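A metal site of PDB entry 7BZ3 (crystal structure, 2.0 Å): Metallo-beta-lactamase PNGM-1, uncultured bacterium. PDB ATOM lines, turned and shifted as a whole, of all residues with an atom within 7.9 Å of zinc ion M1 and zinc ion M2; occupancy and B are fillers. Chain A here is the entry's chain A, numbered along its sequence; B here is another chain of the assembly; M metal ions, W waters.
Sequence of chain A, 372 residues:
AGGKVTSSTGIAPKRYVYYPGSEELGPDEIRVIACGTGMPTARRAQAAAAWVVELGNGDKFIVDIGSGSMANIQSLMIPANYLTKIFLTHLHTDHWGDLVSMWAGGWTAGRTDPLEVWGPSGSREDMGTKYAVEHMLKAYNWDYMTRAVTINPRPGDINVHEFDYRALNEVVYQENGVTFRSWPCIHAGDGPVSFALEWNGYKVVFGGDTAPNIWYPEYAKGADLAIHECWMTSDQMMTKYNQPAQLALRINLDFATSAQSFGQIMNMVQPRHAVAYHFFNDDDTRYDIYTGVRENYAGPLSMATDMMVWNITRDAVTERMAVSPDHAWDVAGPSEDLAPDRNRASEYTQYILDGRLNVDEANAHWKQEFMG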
ATOM      1  N   GLY A  38     -13.768 -12.314  -9.244  1.00  0.00           N
ATOM      2  CA  GLY A  38     -13.997 -13.778  -9.289  1.00  0.00           C
ATOM      3  C   GLY A  38     -15.369 -14.152  -8.791  1.00  0.00           C
ATOM      4  O   GLY A  38     -16.301 -13.413  -9.076  1.00  0.00           O
ATOM      5  N   MET A  39     -15.473 -15.225  -8.016  1.00  0.00           N
ATOM      6  CA  MET A  39     -16.754 -15.912  -7.709  1.00  0.00           C
ATOM      7  C   MET A  39     -16.884 -16.186  -6.205  1.00  0.00           C
ATOM      8  O   MET A  39     -15.986 -15.881  -5.439  1.00  0.00           O
ATOM      9  CB  MET A  39     -16.790 -17.248  -8.478  1.00  0.00           C
ATOM     10  CG  MET A  39     -16.640 -17.095  -9.997  1.00  0.00           C
ATOM     11  SD  MET A  39     -18.240 -16.753 -10.727  1.00  0.00           S
ATOM     12  CE  MET A  39     -19.029 -18.368 -10.648  1.00  0.00           C
ATOM     13  N   PRO A  40     -17.992 -16.801  -5.735  1.00  0.00           N
ATOM     14  CA  PRO A  40     -18.046 -17.255  -4.343  1.00  0.00           C
ATOM     15  C   PRO A  40     -17.060 -18.418  -4.096  1.00  0.00           C
ATOM     16  O   PRO A  40     -16.759 -18.665  -2.936  1.00  0.00           O
ATOM     17  CB  PRO A  40     -19.501 -17.662  -4.095  1.00  0.00           C
ATOM     18  CG  PRO A  40     -20.276 -17.240  -5.344  1.00  0.00           C
ATOM     19  CD  PRO A  40     -19.254 -17.034  -6.459  1.00  0.00           C
ATOM     20  N   ALA A  48     -12.774 -12.452  -4.680  1.00  0.00           N
ATOM     21  CA  ALA A  48     -14.201 -12.035  -4.836  1.00  0.00           C
ATOM     22  C   ALA A  48     -14.291 -10.507  -5.052  1.00  0.00           C
ATOM     23  O   ALA A  48     -13.346  -9.785  -4.654  1.00  0.00           O
ATOM     24  CB  ALA A  48     -15.002 -12.457  -3.644  1.00  0.00           C
ATOM     25  N   ALA A  49     -15.444 -10.014  -5.516  1.00  0.00           N
ATOM     26  CA  ALA A  49     -15.652  -8.676  -6.127  1.00  0.00           C
ATOM     27  C   ALA A  49     -15.180  -7.537  -5.210  1.00  0.00           C
ATOM     28  O   ALA A  49     -15.660  -7.426  -4.081  1.00  0.00           O
ATOM     29  CB  ALA A  49     -17.105  -8.516  -6.511  1.00  0.00           C
ATOM     30  N   ASP A  64     -17.763  -2.713  -3.183  1.00  0.00           N
ATOM     31  CA  ASP A  64     -17.719  -4.165  -2.881  1.00  0.00           C
ATOM     32  C   ASP A  64     -16.376  -4.522  -2.235  1.00  0.00           C
ATOM     33  O   ASP A  64     -15.355  -3.813  -2.461  1.00  0.00           O
ATOM     34  CB  ASP A  64     -18.106  -5.014  -4.091  1.00  0.00           C
ATOM     35  CG  ASP A  64     -19.608  -4.998  -4.396  1.00  0.00           C
ATOM     36  OD1 ASP A  64     -20.377  -4.395  -3.576  1.00  0.00           O
ATOM     37  OD2 ASP A  64     -20.019  -5.573  -5.466  1.00  0.00           O
ATOM     38  N   THR A  89     -23.082  -3.402  -3.177  1.00  0.00           N
ATOM     39  CA  THR A  89     -24.167  -3.593  -4.195  1.00  0.00           C
ATOM     40  C   THR A  89     -25.229  -4.491  -3.581  1.00  0.00           C
ATOM     41  O   THR A  89     -26.419  -4.276  -3.896  1.00  0.00           O
ATOM     42  CB  THR A  89     -23.600  -4.141  -5.511  1.00  0.00           C
ATOM     43  OG1 THR A  89     -22.912  -5.381  -5.305  1.00  0.00           O
ATOM     44  CG2 THR A  89     -22.636  -3.181  -6.165  1.00  0.00           C
ATOM     45  N   HIS A  90     -24.784  -5.443  -2.738  1.00  0.00           N
ATOM     46  CA  HIS A  90     -25.627  -6.504  -2.132  1.00  0.00           C
ATOM     47  C   HIS A  90     -24.852  -7.325  -1.096  1.00  0.00           C
ATOM     48  O   HIS A  90     -23.622  -7.120  -0.893  1.00  0.00           O
ATOM     49  CB  HIS A  90     -26.325  -7.328  -3.217  1.00  0.00           C
ATOM     50  CG  HIS A  90     -25.467  -8.285  -3.965  1.00  0.00           C
ATOM     51  ND1 HIS A  90     -24.435  -7.878  -4.775  1.00  0.00           N
ATOM     52  CD2 HIS A  90     -25.556  -9.625  -4.079  1.00  0.00           C
ATOM     53  CE1 HIS A  90     -23.895  -8.945  -5.313  1.00  0.00           C
ATOM     54  NE2 HIS A  90     -24.558 -10.022  -4.903  1.00  0.00           N
ATOM     55  N   LEU A  91     -25.584  -8.216  -0.436  1.00  0.00           N
ATOM     56  CA  LEU A  91     -25.114  -8.909   0.810  1.00  0.00           C
ATOM     57  C   LEU A  91     -24.694 -10.358   0.576  1.00  0.00           C
ATOM     58  O   LEU A  91     -24.626 -11.108   1.581  1.00  0.00           O
ATOM     59  CB  LEU A  91     -26.227  -8.747   1.842  1.00  0.00           C
ATOM     60  CG  LEU A  91     -26.475  -7.298   2.219  1.00  0.00           C
ATOM     61  CD1 LEU A  91     -27.765  -7.182   2.962  1.00  0.00           C
ATOM     62  CD2 LEU A  91     -25.304  -6.711   2.991  1.00  0.00           C
ATOM     63  N   HIS A  92     -24.272 -10.750  -0.624  1.00  0.00           N
ATOM     64  CA  HIS A  92     -23.535 -12.042  -0.838  1.00  0.00           C
ATOM     65  C   HIS A  92     -22.131 -11.952  -0.239  1.00  0.00           C
ATOM     66  O   HIS A  92     -21.527 -10.898  -0.335  1.00  0.00           O
ATOM     67  CB  HIS A  92     -23.476 -12.465  -2.285  1.00  0.00           C
ATOM     68  CG  HIS A  92     -24.673 -13.230  -2.747  1.00  0.00           C
ATOM     69  ND1 HIS A  92     -25.210 -13.026  -3.986  1.00  0.00           N
ATOM     70  CD2 HIS A  92     -25.433 -14.153  -2.146  1.00  0.00           C
ATOM     71  CE1 HIS A  92     -26.228 -13.843  -4.158  1.00  0.00           C
ATOM     72  NE2 HIS A  92     -26.395 -14.542  -3.038  1.00  0.00           N
ATOM     73  N   THR A  93     -21.609 -13.060   0.282  1.00  0.00           N
ATOM     74  CA  THR A  93     -20.225 -13.129   0.842  1.00  0.00           C
ATOM     75  C   THR A  93     -19.197 -12.586  -0.189  1.00  0.00           C
ATOM     76  O   THR A  93     -18.287 -11.886   0.237  1.00  0.00           O
ATOM     77  CB  THR A  93     -19.833 -14.555   1.245  1.00  0.00           C
ATOM     78  OG1 THR A  93     -19.985 -15.414   0.108  1.00  0.00           O
ATOM     79  CG2 THR A  93     -20.624 -15.089   2.418  1.00  0.00           C
ATOM     80  N   ASP A  94     -19.357 -12.862  -1.498  1.00  0.00           N
ATOM     81  CA  ASP A  94     -18.362 -12.500  -2.546  1.00  0.00           C
ATOM     82  C   ASP A  94     -18.395 -10.982  -2.839  1.00  0.00           C
ATOM     83  O   ASP A  94     -17.601 -10.592  -3.711  1.00  0.00           O
ATOM     84  CB  ASP A  94     -18.485 -13.322  -3.850  1.00  0.00           C
ATOM     85  CG  ASP A  94     -19.828 -13.271  -4.567  1.00  0.00           C
ATOM     86  OD1 ASP A  94     -20.854 -13.523  -3.932  1.00  0.00           O
ATOM     87  OD2 ASP A  94     -19.836 -12.961  -5.774  1.00  0.00           O
ATOM     88  N   HIS A  95     -19.201 -10.194  -2.100  1.00  0.00           N
ATOM     89  CA  HIS A  95     -19.293  -8.715  -2.213  1.00  0.00           C
ATOM     90  C   HIS A  95     -19.020  -7.958  -0.913  1.00  0.00           C
ATOM     91  O   HIS A  95     -18.762  -6.781  -1.028  1.00  0.00           O
ATOM     92  CB  HIS A  95     -20.663  -8.298  -2.776  1.00  0.00           C
ATOM     93  CG  HIS A  95     -20.837  -8.835  -4.139  1.00  0.00           C
ATOM     94  ND1 HIS A  95     -20.499  -8.085  -5.256  1.00  0.00           N
ATOM     95  CD2 HIS A  95     -21.103 -10.095  -4.556  1.00  0.00           C
ATOM     96  CE1 HIS A  95     -20.691  -8.827  -6.320  1.00  0.00           C
ATOM     97  NE2 HIS A  95     -21.056 -10.086  -5.922  1.00  0.00           N
ATOM     98  N   HIS A 187     -31.461 -10.344  -8.713  1.00  0.00           N
ATOM     99  CA  HIS A 187     -30.386 -11.236  -8.223  1.00  0.00           C
ATOM    100  C   HIS A 187     -30.792 -11.866  -6.890  1.00  0.00           C
ATOM    101  O   HIS A 187     -30.744 -11.168  -5.825  1.00  0.00           O
ATOM    102  CB  HIS A 187     -29.086 -10.444  -8.232  1.00  0.00           C
ATOM    103  CG  HIS A 187     -27.915 -11.212  -7.758  1.00  0.00           C
ATOM    104  ND1 HIS A 187     -27.394 -12.293  -8.453  1.00  0.00           N
ATOM    105  CD2 HIS A 187     -27.172 -11.097  -6.639  1.00  0.00           C
ATOM    106  CE1 HIS A 187     -26.353 -12.769  -7.798  1.00  0.00           C
ATOM    107  NE2 HIS A 187     -26.220 -12.052  -6.685  1.00  0.00           N
ATOM    108  N   ALA A 188     -31.173 -13.156  -6.959  1.00  0.00           N
ATOM    109  CA  ALA A 188     -31.435 -14.069  -5.818  1.00  0.00           C
ATOM    110  C   ALA A 188     -32.699 -13.623  -5.078  1.00  0.00           C
ATOM    111  O   ALA A 188     -33.525 -14.494  -4.732  1.00  0.00           O
ATOM    112  CB  ALA A 188     -30.219 -14.124  -4.926  1.00  0.00           C
ATOM    113  N   PRO A 192     -30.451  -6.152  -3.958  1.00  0.00           N
ATOM    114  CA  PRO A 192     -29.282  -5.778  -4.744  1.00  0.00           C
ATOM    115  C   PRO A 192     -29.483  -4.617  -5.711  1.00  0.00           C
ATOM    116  O   PRO A 192     -30.579  -4.438  -6.270  1.00  0.00           O
ATOM    117  CB  PRO A 192     -28.961  -7.041  -5.563  1.00  0.00           C
ATOM    118  CG  PRO A 192     -29.498  -8.170  -4.698  1.00  0.00           C
ATOM    119  CD  PRO A 192     -30.773  -7.585  -4.132  1.00  0.00           C
ATOM    120  N   GLY A 208     -22.592  -4.440 -10.046  1.00  0.00           N
ATOM    121  CA  GLY A 208     -22.885  -5.497  -9.053  1.00  0.00           C
ATOM    122  C   GLY A 208     -23.274  -6.800  -9.725  1.00  0.00           C
ATOM    123  O   GLY A 208     -22.701  -7.146 -10.774  1.00  0.00           O
ATOM    124  N   ASP A 209     -24.252  -7.504  -9.178  1.00  0.00           N
ATOM    125  CA  ASP A 209     -24.754  -8.739  -9.799  1.00  0.00           C
ATOM    126  C   ASP A 209     -26.195  -8.542 -10.244  1.00  0.00           C
ATOM    127  O   ASP A 209     -26.983  -8.068  -9.420  1.00  0.00           O
ATOM    128  CB  ASP A 209     -24.724  -9.915  -8.845  1.00  0.00           C
ATOM    129  CG  ASP A 209     -23.325 -10.332  -8.441  1.00  0.00           C
ATOM    130  OD1 ASP A 209     -22.348  -9.585  -8.745  1.00  0.00           O
ATOM    131  OD2 ASP A 209     -23.238 -11.368  -7.788  1.00  0.00           O
ATOM    132  N   THR A 210     -26.513  -9.005 -11.448  1.00  0.00           N
ATOM    133  CA  THR A 210     -27.903  -8.970 -11.953  1.00  0.00           C
ATOM    134  C   THR A 210     -28.065  -9.943 -13.120  1.00  0.00           C
ATOM    135  O   THR A 210     -27.073 -10.194 -13.804  1.00  0.00           O
ATOM    136  CB  THR A 210     -28.274  -7.535 -12.360  1.00  0.00           C
ATOM    137  OG1 THR A 210     -29.665  -7.511 -12.626  1.00  0.00           O
ATOM    138  CG2 THR A 210     -27.516  -7.052 -13.576  1.00  0.00           C
ATOM    139  N   GLU A 229     -21.720  -7.751 -14.654  1.00  0.00           N
ATOM    140  CA  GLU A 229     -21.509  -9.206 -14.535  1.00  0.00           C
ATOM    141  C   GLU A 229     -21.560  -9.816 -15.959  1.00  0.00           C
ATOM    142  O   GLU A 229     -22.426  -9.406 -16.800  1.00  0.00           O
ATOM    143  CB  GLU A 229     -22.513  -9.745 -13.524  1.00  0.00           C
ATOM    144  CG  GLU A 229     -22.799 -11.220 -13.615  1.00  0.00           C
ATOM    145  CD  GLU A 229     -24.181 -11.578 -13.080  1.00  0.00           C
ATOM    146  OE1 GLU A 229     -24.621 -11.003 -12.030  1.00  0.00           O
ATOM    147  OE2 GLU A 229     -24.824 -12.443 -13.739  1.00  0.00           O
ATOM    148  N   TRP A 231     -21.114 -13.896 -17.402  1.00  0.00           N
ATOM    149  CA  TRP A 231     -21.041 -15.264 -16.823  1.00  0.00           C
ATOM    150  C   TRP A 231     -20.209 -16.191 -17.704  1.00  0.00           C
ATOM    151  O   TRP A 231     -20.154 -15.983 -18.911  1.00  0.00           O
ATOM    152  CB  TRP A 231     -22.425 -15.847 -16.549  1.00  0.00           C
ATOM    153  CG  TRP A 231     -22.439 -16.687 -15.310  1.00  0.00           C
ATOM    154  CD1 TRP A 231     -22.376 -18.046 -15.213  1.00  0.00           C
ATOM    155  CD2 TRP A 231     -22.439 -16.187 -13.960  1.00  0.00           C
ATOM    156  NE1 TRP A 231     -22.367 -18.420 -13.894  1.00  0.00           N
ATOM    157  CE2 TRP A 231     -22.417 -17.308 -13.100  1.00  0.00           C
ATOM    158  CE3 TRP A 231     -22.454 -14.915 -13.391  1.00  0.00           C
ATOM    159  CZ2 TRP A 231     -22.428 -17.182 -11.711  1.00  0.00           C
ATOM    160  CZ3 TRP A 231     -22.469 -14.791 -12.027  1.00  0.00           C
ATOM    161  CH2 TRP A 231     -22.457 -15.915 -11.198  1.00  0.00           C
ATOM    162  N   TYR A 277     -16.903  -8.765 -15.847  1.00  0.00           N
ATOM    163  CA  TYR A 277     -16.318  -9.331 -14.608  1.00  0.00           C
ATOM    164  C   TYR A 277     -17.242 -10.433 -14.081  1.00  0.00           C
ATOM    165  O   TYR A 277     -18.318 -10.710 -14.678  1.00  0.00           O
ATOM    166  CB  TYR A 277     -15.998  -8.191 -13.614  1.00  0.00           C
ATOM    167  CG  TYR A 277     -17.029  -7.995 -12.543  1.00  0.00           C
ATOM    168  CD1 TYR A 277     -18.306  -7.580 -12.868  1.00  0.00           C
ATOM    169  CD2 TYR A 277     -16.775  -8.296 -11.216  1.00  0.00           C
ATOM    170  CE1 TYR A 277     -19.289  -7.427 -11.910  1.00  0.00           C
ATOM    171  CE2 TYR A 277     -17.746  -8.118 -10.225  1.00  0.00           C
ATOM    172  CZ  TYR A 277     -19.015  -7.689 -10.582  1.00  0.00           C
ATOM    173  OH  TYR A 277     -20.017  -7.529  -9.660  1.00  0.00           O
ATOM    174  N   HIS A 278     -16.766 -11.121 -13.052  1.00  0.00           N
ATOM    175  CA  HIS A 278     -17.509 -12.109 -12.233  1.00  0.00           C
ATOM    176  C   HIS A 278     -17.495 -13.473 -12.943  1.00  0.00           C
ATOM    177  O   HIS A 278     -18.502 -14.212 -12.864  1.00  0.00           O
ATOM    178  CB  HIS A 278     -18.919 -11.596 -11.942  1.00  0.00           C
ATOM    179  CG  HIS A 278     -19.478 -12.070 -10.646  1.00  0.00           C
ATOM    180  ND1 HIS A 278     -19.441 -13.418 -10.273  1.00  0.00           N
ATOM    181  CD2 HIS A 278     -20.045 -11.392  -9.622  1.00  0.00           C
ATOM    182  CE1 HIS A 278     -19.987 -13.525  -9.056  1.00  0.00           C
ATOM    183  NE2 HIS A 278     -20.387 -12.279  -8.649  1.00  0.00           N
ATOM    184  N   TRP B 142     -29.611 -12.335   4.584  1.00  0.00           N
ATOM    185  CA  TRP B 142     -30.082 -12.080   3.200  1.00  0.00           C
ATOM    186  C   TRP B 142     -29.634 -13.260   2.321  1.00  0.00           C
ATOM    187  O   TRP B 142     -30.529 -13.892   1.664  1.00  0.00           O
ATOM    188  CB  TRP B 142     -29.617 -10.715   2.688  1.00  0.00           C
ATOM    189  CG  TRP B 142     -30.144 -10.448   1.314  1.00  0.00           C
ATOM    190  CD1 TRP B 142     -31.333  -9.870   1.010  1.00  0.00           C
ATOM    191  CD2 TRP B 142     -29.528 -10.791   0.056  1.00  0.00           C
ATOM    192  NE1 TRP B 142     -31.504  -9.820  -0.349  1.00  0.00           N
ATOM    193  CE2 TRP B 142     -30.421 -10.381  -0.959  1.00  0.00           C
ATOM    194  CE3 TRP B 142     -28.328 -11.416  -0.315  1.00  0.00           C
ATOM    195  CZ2 TRP B 142     -30.158 -10.589  -2.308  1.00  0.00           C
ATOM    196  CZ3 TRP B 142     -28.068 -11.615  -1.661  1.00  0.00           C
ATOM    197  CH2 TRP B 142     -28.979 -11.214  -2.636  1.00  0.00           C
ATOM    198  N   ASP B 143     -28.338 -13.595   2.359  1.00  0.00           N
ATOM    199  CA  ASP B 143     -27.673 -14.739   1.653  1.00  0.00           C
ATOM    200  C   ASP B 143     -28.428 -16.051   1.932  1.00  0.00           C
ATOM    201  O   ASP B 143     -28.850 -16.719   0.955  1.00  0.00           O
ATOM    202  CB  ASP B 143     -26.207 -14.910   2.079  1.00  0.00           C
ATOM    203  CG  ASP B 143     -25.386 -15.849   1.192  1.00  0.00           C
ATOM    204  OD1 ASP B 143     -25.981 -16.567   0.387  1.00  0.00           O
ATOM    205  OD2 ASP B 143     -24.157 -15.791   1.249  1.00  0.00           O
ATOM    206  N   ARG B 147     -31.012 -17.865  -0.873  1.00  0.00           N
ATOM    207  CA  ARG B 147     -30.475 -19.166  -1.379  1.00  0.00           C
ATOM    208  C   ARG B 147     -31.420 -20.321  -1.025  1.00  0.00           C
ATOM    209  O   ARG B 147     -31.558 -21.210  -1.886  1.00  0.00           O
ATOM    210  CB  ARG B 147     -29.110 -19.505  -0.764  1.00  0.00           C
ATOM    211  CG  ARG B 147     -28.444 -20.743  -1.362  1.00  0.00           C
ATOM    212  CD  ARG B 147     -26.954 -20.747  -1.098  1.00  0.00           C
ATOM    213  NE  ARG B 147     -26.315 -19.578  -1.717  1.00  0.00           N
ATOM    214  CZ  ARG B 147     -25.144 -19.036  -1.334  1.00  0.00           C
ATOM    215  NH1 ARG B 147     -24.472 -19.557  -0.324  1.00  0.00           N
ATOM    216  NH2 ARG B 147     -24.668 -17.967  -1.966  1.00  0.00           N
HETATM  217 ZN    ZN M   1     -24.385 -12.017  -5.696  1.00  0.00          ZN
HETATM  218 ZN    ZN M   2     -21.350 -11.882  -6.953  1.00  0.00          ZN
HETATM  219  O   HOH W   1     -22.693 -12.859  -5.972  1.00  0.00           O
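Zinc ion M2 is bound by water W1 (1.9 Å).
Zinc ion M2 is bound by NE2 of His 278.
Zinc ion M2 is bound by a ring nitrogen (NE2) of His 95, 2.1 Å away.
Zinc ion M2 is bound by OD2 of Asp 209 (2.1 Å).
OD2 of Asp 94 is bound to zinc ion M2 (2.2 Å).
Zinc ion M2 has five donor atoms within binding distance.
Four residues have an atom within 4 Å of zinc ion M2: Asp 94, His 95, Asp 209 and His 278.
The nearest printed residue that does not touch zinc ion M2 is His 90 (4.2 Å).
Of the 26 residues printed, 5 come within 4 Å of zinc ion M1.
Water W1 is bound to zinc ion M1 (1.9 Å).
NE2 of His 187 binds zinc ion M1 (2.1 Å).
ND1 of His 92 is bound to zinc ion M1 (2.2 Å).
A ring nitrogen (NE2) of His 90 binds zinc ion M1, 2.2 Å away.
OD2 of Asp 209 is bound to zinc ion M1.
ND1 of His 278 lies within hydrogen-bond range of O of Gly 38, 3.4 Å away.
ND1 of His 278 sits at hydrogen-bond distance from SD of Met 39.
OH of Tyr 277 sits at hydrogen-bond distance from OD1 of Asp 209 (3.2 Å).
A ring nitrogen (ND1) of His 90 sits at hydrogen-bond distance from the side-chain hydroxyl (OG1) of Thr 89, at 3.0 Å.
O of Asp 94 sits at hydrogen-bond distance from N of Ala 49 (2.9 Å).
ND1 of His 95 lies within hydrogen-bond range of OD2 of Asp 64 (2.6 Å).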
